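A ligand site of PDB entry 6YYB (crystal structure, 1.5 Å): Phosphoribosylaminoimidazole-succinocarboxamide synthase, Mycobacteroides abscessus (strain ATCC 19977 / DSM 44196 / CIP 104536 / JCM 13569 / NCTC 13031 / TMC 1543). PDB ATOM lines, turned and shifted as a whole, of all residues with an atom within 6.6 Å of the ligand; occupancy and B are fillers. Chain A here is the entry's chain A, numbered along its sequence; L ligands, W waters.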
ATOM      1  N   VAL A  20      -4.354   0.872  18.038  1.00  0.00           N
ATOM      2  CA  VAL A  20      -4.620   1.341  16.681  1.00  0.00           C
ATOM      3  C   VAL A  20      -5.663   2.454  16.603  1.00  0.00           C
ATOM      4  O   VAL A  20      -5.750   3.160  15.601  1.00  0.00           O
ATOM      5  CB  VAL A  20      -5.044   0.179  15.770  1.00  0.00           C
ATOM      6  CG1 VAL A  20      -3.891  -0.797  15.612  1.00  0.00           C
ATOM      7  CG2 VAL A  20      -6.284  -0.503  16.319  1.00  0.00           C
ATOM      8  N   ALA A  21      -6.472   2.599  17.652  1.00  0.00           N
ATOM      9  CA  ALA A  21      -7.457   3.669  17.679  1.00  0.00           C
ATOM     10  C   ALA A  21      -7.898   3.996  19.095  1.00  0.00           C
ATOM     11  O   ALA A  21      -7.930   3.129  19.975  1.00  0.00           O
ATOM     12  CB  ALA A  21      -8.673   3.303  16.811  1.00  0.00           C
ATOM     13  N   SER A  22      -8.248   5.263  19.297  1.00  0.00           N
ATOM     14  CA  SER A  22      -8.869   5.713  20.540  1.00  0.00           C
ATOM     15  C   SER A  22     -10.100   6.564  20.254  1.00  0.00           C
ATOM     16  O   SER A  22     -10.078   7.419  19.370  1.00  0.00           O
ATOM     17  CB  SER A  22      -7.883   6.499  21.402  1.00  0.00           C
ATOM     18  OG  SER A  22      -6.968   5.645  22.063  1.00  0.00           O
ATOM     19  N   GLY A  23     -11.158   6.318  21.021  1.00  0.00           N
ATOM     20  CA  GLY A  23     -12.323   7.175  21.036  1.00  0.00           C
ATOM     21  C   GLY A  23     -12.371   7.877  22.385  1.00  0.00           C
ATOM     22  O   GLY A  23     -11.448   7.736  23.190  1.00  0.00           O
ATOM     23  N   ARG A  26     -13.431   4.744  24.616  1.00  0.00           N
ATOM     24  CA  ARG A  26     -13.118   3.405  24.120  1.00  0.00           C
ATOM     25  C   ARG A  26     -11.738   3.334  23.466  1.00  0.00           C
ATOM     26  O   ARG A  26     -11.187   4.341  23.012  1.00  0.00           O
ATOM     27  CB  ARG A  26     -14.132   2.929  23.079  1.00  0.00           C
ATOM     28  CG  ARG A  26     -15.526   3.453  23.247  1.00  0.00           C
ATOM     29  CD  ARG A  26     -16.388   2.925  22.123  1.00  0.00           C
ATOM     30  NE  ARG A  26     -16.180   3.593  20.843  1.00  0.00           N
ATOM     31  CZ  ARG A  26     -16.943   3.345  19.780  1.00  0.00           C
ATOM     32  NH1 ARG A  26     -17.919   2.453  19.884  1.00  0.00           N
ATOM     33  NH2 ARG A  26     -16.750   3.970  18.627  1.00  0.00           N
ATOM     34  N   GLU A  27     -11.200   2.132  23.380  1.00  0.00           N
ATOM     35  CA  GLU A  27      -9.894   1.933  22.752  1.00  0.00           C
ATOM     36  C   GLU A  27      -9.915   0.706  21.873  1.00  0.00           C
ATOM     37  O   GLU A  27     -10.700  -0.204  22.093  1.00  0.00           O
ATOM     38  CB  GLU A  27      -8.811   1.786  23.823  1.00  0.00           C
ATOM     39  CG  GLU A  27      -8.640   2.998  24.715  1.00  0.00           C
ATOM     40  CD  GLU A  27      -7.679   2.725  25.854  1.00  0.00           C
ATOM     41  OE1 GLU A  27      -7.532   1.549  26.238  1.00  0.00           O
ATOM     42  OE2 GLU A  27      -7.061   3.697  26.340  1.00  0.00           O
ATOM     43  N   LEU A  28      -9.028   0.679  20.878  1.00  0.00           N
ATOM     44  CA  LEU A  28      -8.945  -0.465  19.978  1.00  0.00           C
ATOM     45  C   LEU A  28      -7.490  -0.908  19.794  1.00  0.00           C
ATOM     46  O   LEU A  28      -6.605  -0.087  19.584  1.00  0.00           O
ATOM     47  CB  LEU A  28      -9.567  -0.101  18.624  1.00  0.00           C
ATOM     48  CG  LEU A  28      -9.950  -1.225  17.663  1.00  0.00           C
ATOM     49  CD1 LEU A  28     -11.064  -2.078  18.254  1.00  0.00           C
ATOM     50  CD2 LEU A  28     -10.359  -0.632  16.346  1.00  0.00           C
ATOM     51  N   LEU A  36      -8.956  -8.027  16.524  1.00  0.00           N
ATOM     52  CA  LEU A  36      -8.737  -6.842  17.339  1.00  0.00           C
ATOM     53  C   LEU A  36      -9.225  -7.075  18.775  1.00  0.00           C
ATOM     54  O   LEU A  36      -9.954  -8.019  19.043  1.00  0.00           O
ATOM     55  CB  LEU A  36      -9.465  -5.634  16.741  1.00  0.00           C
ATOM     56  CG  LEU A  36      -9.185  -5.368  15.270  1.00  0.00           C
ATOM     57  CD1 LEU A  36     -10.146  -4.325  14.739  1.00  0.00           C
ATOM     58  CD2 LEU A  36      -7.759  -4.889  15.094  1.00  0.00           C
ATOM     59  N   PHE A  38     -11.361  -4.927  21.451  1.00  0.00           N
ATOM     60  CA  PHE A  38     -12.226  -3.774  21.637  1.00  0.00           C
ATOM     61  C   PHE A  38     -12.349  -3.490  23.138  1.00  0.00           C
ATOM     62  O   PHE A  38     -12.907  -4.308  23.863  1.00  0.00           O
ATOM     63  CB  PHE A  38     -13.602  -4.048  20.997  1.00  0.00           C
ATOM     64  CG  PHE A  38     -14.484  -2.840  20.837  1.00  0.00           C
ATOM     65  CD1 PHE A  38     -14.970  -2.146  21.942  1.00  0.00           C
ATOM     66  CD2 PHE A  38     -14.852  -2.410  19.570  1.00  0.00           C
ATOM     67  CE1 PHE A  38     -15.783  -1.046  21.790  1.00  0.00           C
ATOM     68  CE2 PHE A  38     -15.673  -1.300  19.411  1.00  0.00           C
ATOM     69  CZ  PHE A  38     -16.127  -0.620  20.519  1.00  0.00           C
ATOM     70  N   VAL A  39     -11.841  -2.353  23.583  1.00  0.00           N
ATOM     71  CA  VAL A  39     -11.793  -2.023  25.010  1.00  0.00           C
ATOM     72  C   VAL A  39     -12.690  -0.857  25.405  1.00  0.00           C
ATOM     73  O   VAL A  39     -12.589   0.244  24.843  1.00  0.00           O
ATOM     74  CB  VAL A  39     -10.346  -1.680  25.451  1.00  0.00           C
ATOM     75  CG1 VAL A  39     -10.322  -1.333  26.928  1.00  0.00           C
ATOM     76  CG2 VAL A  39      -9.414  -2.836  25.116  1.00  0.00           C
ATOM     77  N   HIS A  78     -19.259  -9.113  15.069  1.00  0.00           N
ATOM     78  CA  HIS A  78     -17.814  -9.246  14.967  1.00  0.00           C
ATOM     79  C   HIS A  78     -17.185  -9.950  16.159  1.00  0.00           C
ATOM     80  O   HIS A  78     -15.974 -10.103  16.204  1.00  0.00           O
ATOM     81  CB  HIS A  78     -17.170  -7.869  14.730  1.00  0.00           C
ATOM     82  CG  HIS A  78     -17.148  -6.924  15.898  1.00  0.00           C
ATOM     83  ND1 HIS A  78     -18.073  -6.933  16.930  1.00  0.00           N
ATOM     84  CD2 HIS A  78     -16.362  -5.848  16.123  1.00  0.00           C
ATOM     85  CE1 HIS A  78     -17.801  -5.948  17.775  1.00  0.00           C
ATOM     86  NE2 HIS A  78     -16.780  -5.261  17.294  1.00  0.00           N
ATOM     87  N   VAL A  99     -12.508  -9.427  18.793  1.00  0.00           N
ATOM     88  CA  VAL A  99     -13.388  -9.297  17.642  1.00  0.00           C
ATOM     89  C   VAL A  99     -12.656  -9.589  16.314  1.00  0.00           C
ATOM     90  O   VAL A  99     -11.431  -9.525  16.250  1.00  0.00           O
ATOM     91  CB  VAL A  99     -14.032  -7.885  17.601  1.00  0.00           C
ATOM     92  CG1 VAL A  99     -14.834  -7.625  18.879  1.00  0.00           C
ATOM     93  CG2 VAL A  99     -12.991  -6.780  17.368  1.00  0.00           C
ATOM     94  N   ARG A 100     -13.427  -9.929  15.283  1.00  0.00           N
ATOM     95  CA  ARG A 100     -12.860 -10.181  13.951  1.00  0.00           C
ATOM     96  C   ARG A 100     -12.577  -8.875  13.245  1.00  0.00           C
ATOM     97  O   ARG A 100     -13.399  -7.964  13.304  1.00  0.00           O
ATOM     98  CB  ARG A 100     -13.804 -10.982  13.051  1.00  0.00           C
ATOM     99  CG  ARG A 100     -14.645 -12.088  13.654  1.00  0.00           C
ATOM    100  CD  ARG A 100     -15.474 -12.740  12.513  1.00  0.00           C
ATOM    101  NE  ARG A 100     -16.900 -12.451  12.577  1.00  0.00           N
ATOM    102  CZ  ARG A 100     -17.704 -12.386  11.509  1.00  0.00           C
ATOM    103  NH1 ARG A 100     -17.222 -12.551  10.288  1.00  0.00           N
ATOM    104  NH2 ARG A 100     -19.003 -12.139  11.671  1.00  0.00           N
ATOM    105  N   ARG A 101     -11.437  -8.757  12.573  1.00  0.00           N
ATOM    106  CA  ARG A 101     -11.160  -7.548  11.802  1.00  0.00           C
ATOM    107  C   ARG A 101     -12.041  -7.509  10.560  1.00  0.00           C
ATOM    108  O   ARG A 101     -12.100  -8.475   9.828  1.00  0.00           O
ATOM    109  CB  ARG A 101      -9.693  -7.472  11.386  1.00  0.00           C
ATOM    110  CG  ARG A 101      -9.337  -6.117  10.763  1.00  0.00           C
ATOM    111  CD  ARG A 101      -7.938  -6.139  10.167  1.00  0.00           C
ATOM    112  NE  ARG A 101      -7.784  -7.210   9.185  1.00  0.00           N
ATOM    113  CZ  ARG A 101      -8.207  -7.131   7.925  1.00  0.00           C
ATOM    114  NH1 ARG A 101      -8.795  -6.023   7.489  1.00  0.00           N
ATOM    115  NH2 ARG A 101      -8.036  -8.159   7.109  1.00  0.00           N
ATOM    116  N   LEU A 102     -12.713  -6.384  10.353  1.00  0.00           N
ATOM    117  CA  LEU A 102     -13.568  -6.182   9.184  1.00  0.00           C
ATOM    118  C   LEU A 102     -13.144  -4.980   8.369  1.00  0.00           C
ATOM    119  O   LEU A 102     -12.439  -4.100   8.862  1.00  0.00           O
ATOM    120  CB  LEU A 102     -15.010  -6.004   9.627  1.00  0.00           C
ATOM    121  CG  LEU A 102     -15.612  -7.104  10.493  1.00  0.00           C
ATOM    122  CD1 LEU A 102     -16.874  -6.593  11.133  1.00  0.00           C
ATOM    123  CD2 LEU A 102     -15.928  -8.332   9.657  1.00  0.00           C
ATOM    124  N   ASP A 103     -13.588  -4.919   7.123  1.00  0.00           N
ATOM    125  CA  ASP A 103     -13.493  -3.688   6.372  1.00  0.00           C
ATOM    126  C   ASP A 103     -14.699  -2.821   6.756  1.00  0.00           C
ATOM    127  O   ASP A 103     -15.824  -3.068   6.311  1.00  0.00           O
ATOM    128  CB  ASP A 103     -13.450  -3.951   4.873  1.00  0.00           C
ATOM    129  CG  ASP A 103     -12.158  -4.621   4.443  1.00  0.00           C
ATOM    130  OD1 ASP A 103     -11.123  -4.408   5.098  1.00  0.00           O
ATOM    131  OD2 ASP A 103     -12.200  -5.365   3.435  1.00  0.00           O
ATOM    132  N   MET A 104     -14.455  -1.796   7.559  1.00  0.00           N
ATOM    133  CA  MET A 104     -15.550  -0.971   8.075  1.00  0.00           C
ATOM    134  C   MET A 104     -16.185  -0.076   6.999  1.00  0.00           C
ATOM    135  O   MET A 104     -15.494   0.492   6.149  1.00  0.00           O
ATOM    136  CB  MET A 104     -15.056  -0.118   9.232  1.00  0.00           C
ATOM    137  CG  MET A 104     -14.545  -0.935  10.408  1.00  0.00           C
ATOM    138  SD  MET A 104     -15.781  -2.055  11.105  1.00  0.00           S
ATOM    139  CE  MET A 104     -16.933  -0.865  11.814  1.00  0.00           C
ATOM    140  N   GLU A 108     -22.155   6.165   9.852  1.00  0.00           N
ATOM    141  CA  GLU A 108     -22.784   5.996  11.162  1.00  0.00           C
ATOM    142  C   GLU A 108     -24.244   5.645  10.966  1.00  0.00           C
ATOM    143  O   GLU A 108     -25.031   6.487  10.556  1.00  0.00           O
ATOM    144  CB  GLU A 108     -22.652   7.268  12.006  1.00  0.00           C
ATOM    145  CG  GLU A 108     -21.206   7.714  12.172  1.00  0.00           C
ATOM    146  CD  GLU A 108     -20.305   6.581  12.637  1.00  0.00           C
ATOM    147  OE1 GLU A 108     -20.496   6.094  13.773  1.00  0.00           O
ATOM    148  OE2 GLU A 108     -19.418   6.168  11.852  1.00  0.00           O
ATOM    149  N   GLU A 209     -22.028   0.933  13.832  1.00  0.00           N
ATOM    150  CA  GLU A 209     -21.219   0.821  12.628  1.00  0.00           C
ATOM    151  C   GLU A 209     -21.194  -0.631  12.162  1.00  0.00           C
ATOM    152  O   GLU A 209     -21.224  -1.560  12.971  1.00  0.00           O
ATOM    153  CB  GLU A 209     -19.786   1.328  12.848  1.00  0.00           C
ATOM    154  CG  GLU A 209     -19.651   2.843  12.881  1.00  0.00           C
ATOM    155  CD  GLU A 209     -18.227   3.267  13.157  1.00  0.00           C
ATOM    156  OE1 GLU A 209     -17.324   2.401  13.153  1.00  0.00           O
ATOM    157  OE2 GLU A 209     -17.998   4.474  13.398  1.00  0.00           O
ATOM    158  N   LEU A 220     -22.330  -6.658  12.003  1.00  0.00           N
ATOM    159  CA  LEU A 220     -22.459  -5.642  13.053  1.00  0.00           C
ATOM    160  C   LEU A 220     -21.174  -5.578  13.898  1.00  0.00           C
ATOM    161  O   LEU A 220     -20.716  -6.584  14.401  1.00  0.00           O
ATOM    162  CB  LEU A 220     -23.676  -5.956  13.921  1.00  0.00           C
ATOM    163  CG  LEU A 220     -24.133  -4.945  14.977  1.00  0.00           C
ATOM    164  CD1 LEU A 220     -24.419  -3.580  14.403  1.00  0.00           C
ATOM    165  CD2 LEU A 220     -25.359  -5.498  15.678  1.00  0.00           C
ATOM    166  N   ALA A 221     -20.611  -4.382  14.035  1.00  0.00           N
ATOM    167  CA  ALA A 221     -19.253  -4.255  14.584  1.00  0.00           C
ATOM    168  C   ALA A 221     -19.003  -2.927  15.257  1.00  0.00           C
ATOM    169  O   ALA A 221     -18.433  -2.011  14.665  1.00  0.00           O
ATOM    170  CB  ALA A 221     -18.226  -4.443  13.505  1.00  0.00           C
ATOM    171  N   ASP A 222     -19.406  -2.850  16.514  1.00  0.00           N
ATOM    172  CA  ASP A 222     -19.031  -1.746  17.374  1.00  0.00           C
ATOM    173  C   ASP A 222     -19.415  -2.215  18.761  1.00  0.00           C
ATOM    174  O   ASP A 222     -19.249  -3.397  19.075  1.00  0.00           O
ATOM    175  CB  ASP A 222     -19.761  -0.451  16.976  1.00  0.00           C
ATOM    176  CG  ASP A 222     -19.253   0.766  17.738  1.00  0.00           C
ATOM    177  OD1 ASP A 222     -18.013   0.975  17.780  1.00  0.00           O
ATOM    178  OD2 ASP A 222     -20.068   1.510  18.316  1.00  0.00           O
ATOM    179  N   GLU A 223     -19.916  -1.306  19.575  1.00  0.00           N
ATOM    180  CA  GLU A 223     -20.648  -1.673  20.766  1.00  0.00           C
ATOM    181  C   GLU A 223     -22.110  -1.515  20.370  1.00  0.00           C
ATOM    182  O   GLU A 223     -22.436  -0.713  19.493  1.00  0.00           O
ATOM    183  CB  GLU A 223     -20.271  -0.792  21.949  1.00  0.00           C
ATOM    184  CG  GLU A 223     -20.599   0.674  21.754  1.00  0.00           C
ATOM    185  CD  GLU A 223     -20.078   1.526  22.895  1.00  0.00           C
ATOM    186  OE1 GLU A 223     -18.852   1.508  23.117  1.00  0.00           O
ATOM    187  OE2 GLU A 223     -20.884   2.185  23.576  1.00  0.00           O
HETATM  188  C1  LIG L   1     -13.092  -0.392  14.042  1.00  0.00           C
HETATM  189  N1  LIG L   1     -13.696   1.458  15.028  1.00  0.00           N
HETATM  190  C2  LIG L   1     -14.410   2.382  15.846  1.00  0.00           C
HETATM  191  C3  LIG L   1     -13.614   2.455  17.175  1.00  0.00           C
HETATM  192  C4  LIG L   1     -13.099   1.578  19.353  1.00  0.00           C
HETATM  193  C5  LIG L   1     -12.658   3.451  17.329  1.00  0.00           C
HETATM  194  C6  LIG L   1     -12.172   0.589  13.723  1.00  0.00           C
HETATM  195  N2  LIG L   1     -14.307  -5.290  14.025  1.00  0.00           N
HETATM  196  C7  LIG L   1     -13.602  -4.164  13.530  1.00  0.00           C
HETATM  197  C8  LIG L   1     -13.763  -2.890  14.110  1.00  0.00           C
HETATM  198  C9  LIG L   1     -14.713  -2.736  15.271  1.00  0.00           C
HETATM  199  N3  LIG L   1     -15.436  -2.648  16.150  1.00  0.00           N
HETATM  200  C10 LIG L   1     -13.034  -1.820  13.543  1.00  0.00           C
HETATM  201  N4  LIG L   1     -12.214  -2.088  12.501  1.00  0.00           N
HETATM  202  C11 LIG L   1     -12.092  -3.299  11.993  1.00  0.00           C
HETATM  203  N5  LIG L   1     -12.769  -4.312  12.478  1.00  0.00           N
HETATM  204  C12 LIG L   1     -14.043   0.185  14.875  1.00  0.00           C
HETATM  205  C13 LIG L   1     -14.527   3.745  15.166  1.00  0.00           C
HETATM  206  C14 LIG L   1     -13.829   1.512  18.172  1.00  0.00           C
HETATM  207  C15 LIG L   1     -12.154   2.581  19.515  1.00  0.00           C
HETATM  208  C16 LIG L   1     -11.923   3.517  18.519  1.00  0.00           C
HETATM  209  N6  LIG L   1     -12.554   1.734  14.350  1.00  0.00           N
HETATM  210  O   HOH W   1     -11.024  -0.398  10.519  1.00  0.00           O
HETATM  211  O   HOH W   2     -11.038   4.215  13.869  1.00  0.00           O
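The backbone carbonyl oxygen (O) of Arg 100 is in hydrogen-bond range of a nitrogen (N2) of the ligand, at 2.9 Å.
N of Leu 102 is in hydrogen-bond range of N5 of the ligand, at 3.0 Å.
NE2 of His 78 lies within hydrogen-bond range of N3 of the ligand, 3.2 Å away.
O of His 78 sits at hydrogen-bond distance from N of Arg 100 (2.7 Å).
The backbone NH (N) of His 78 is in hydrogen-bond range of the backbone carbonyl oxygen (O) of Leu 220 (3.0 Å).
N of Ala 221 lies within hydrogen-bond range of O of Glu 209 (3.1 Å).
N of Leu 28 sits at hydrogen-bond distance from O of Ala 21, at 2.8 Å.
The backbone carbonyl oxygen of Leu 28 lies within hydrogen-bond range of the backbone NH of Val 20 (2.9 Å).
NH1 of Arg 101 lies within salt-bridge range of OD1 of Asp 103 (3.7 Å).
O of Val 39 sits at hydrogen-bond distance from N of Glu 27, 2.8 Å away.
The side-chain carboxylate (OE1) of Glu 223 is in salt-bridge range of the guanidinium group (NH1) of Arg 26 (3.5 Å).
The backbone carbonyl oxygen of Ala 221 lies close to a nitrogen (N3) of the ligand.
Merely in contact with the ligand: Met 104, Leu 28, Leu 36, Phe 38, Arg 101, Ala 21, Glu 209, Glu 27, Arg 26, Gly 23, Val 99, Asp 222 and Ser 22.
Hydrophobic or aromatic side chains that line the ligand: Ala 21, Leu 28, Leu 36, Phe 38, His 78, Val 99 and Met 104.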
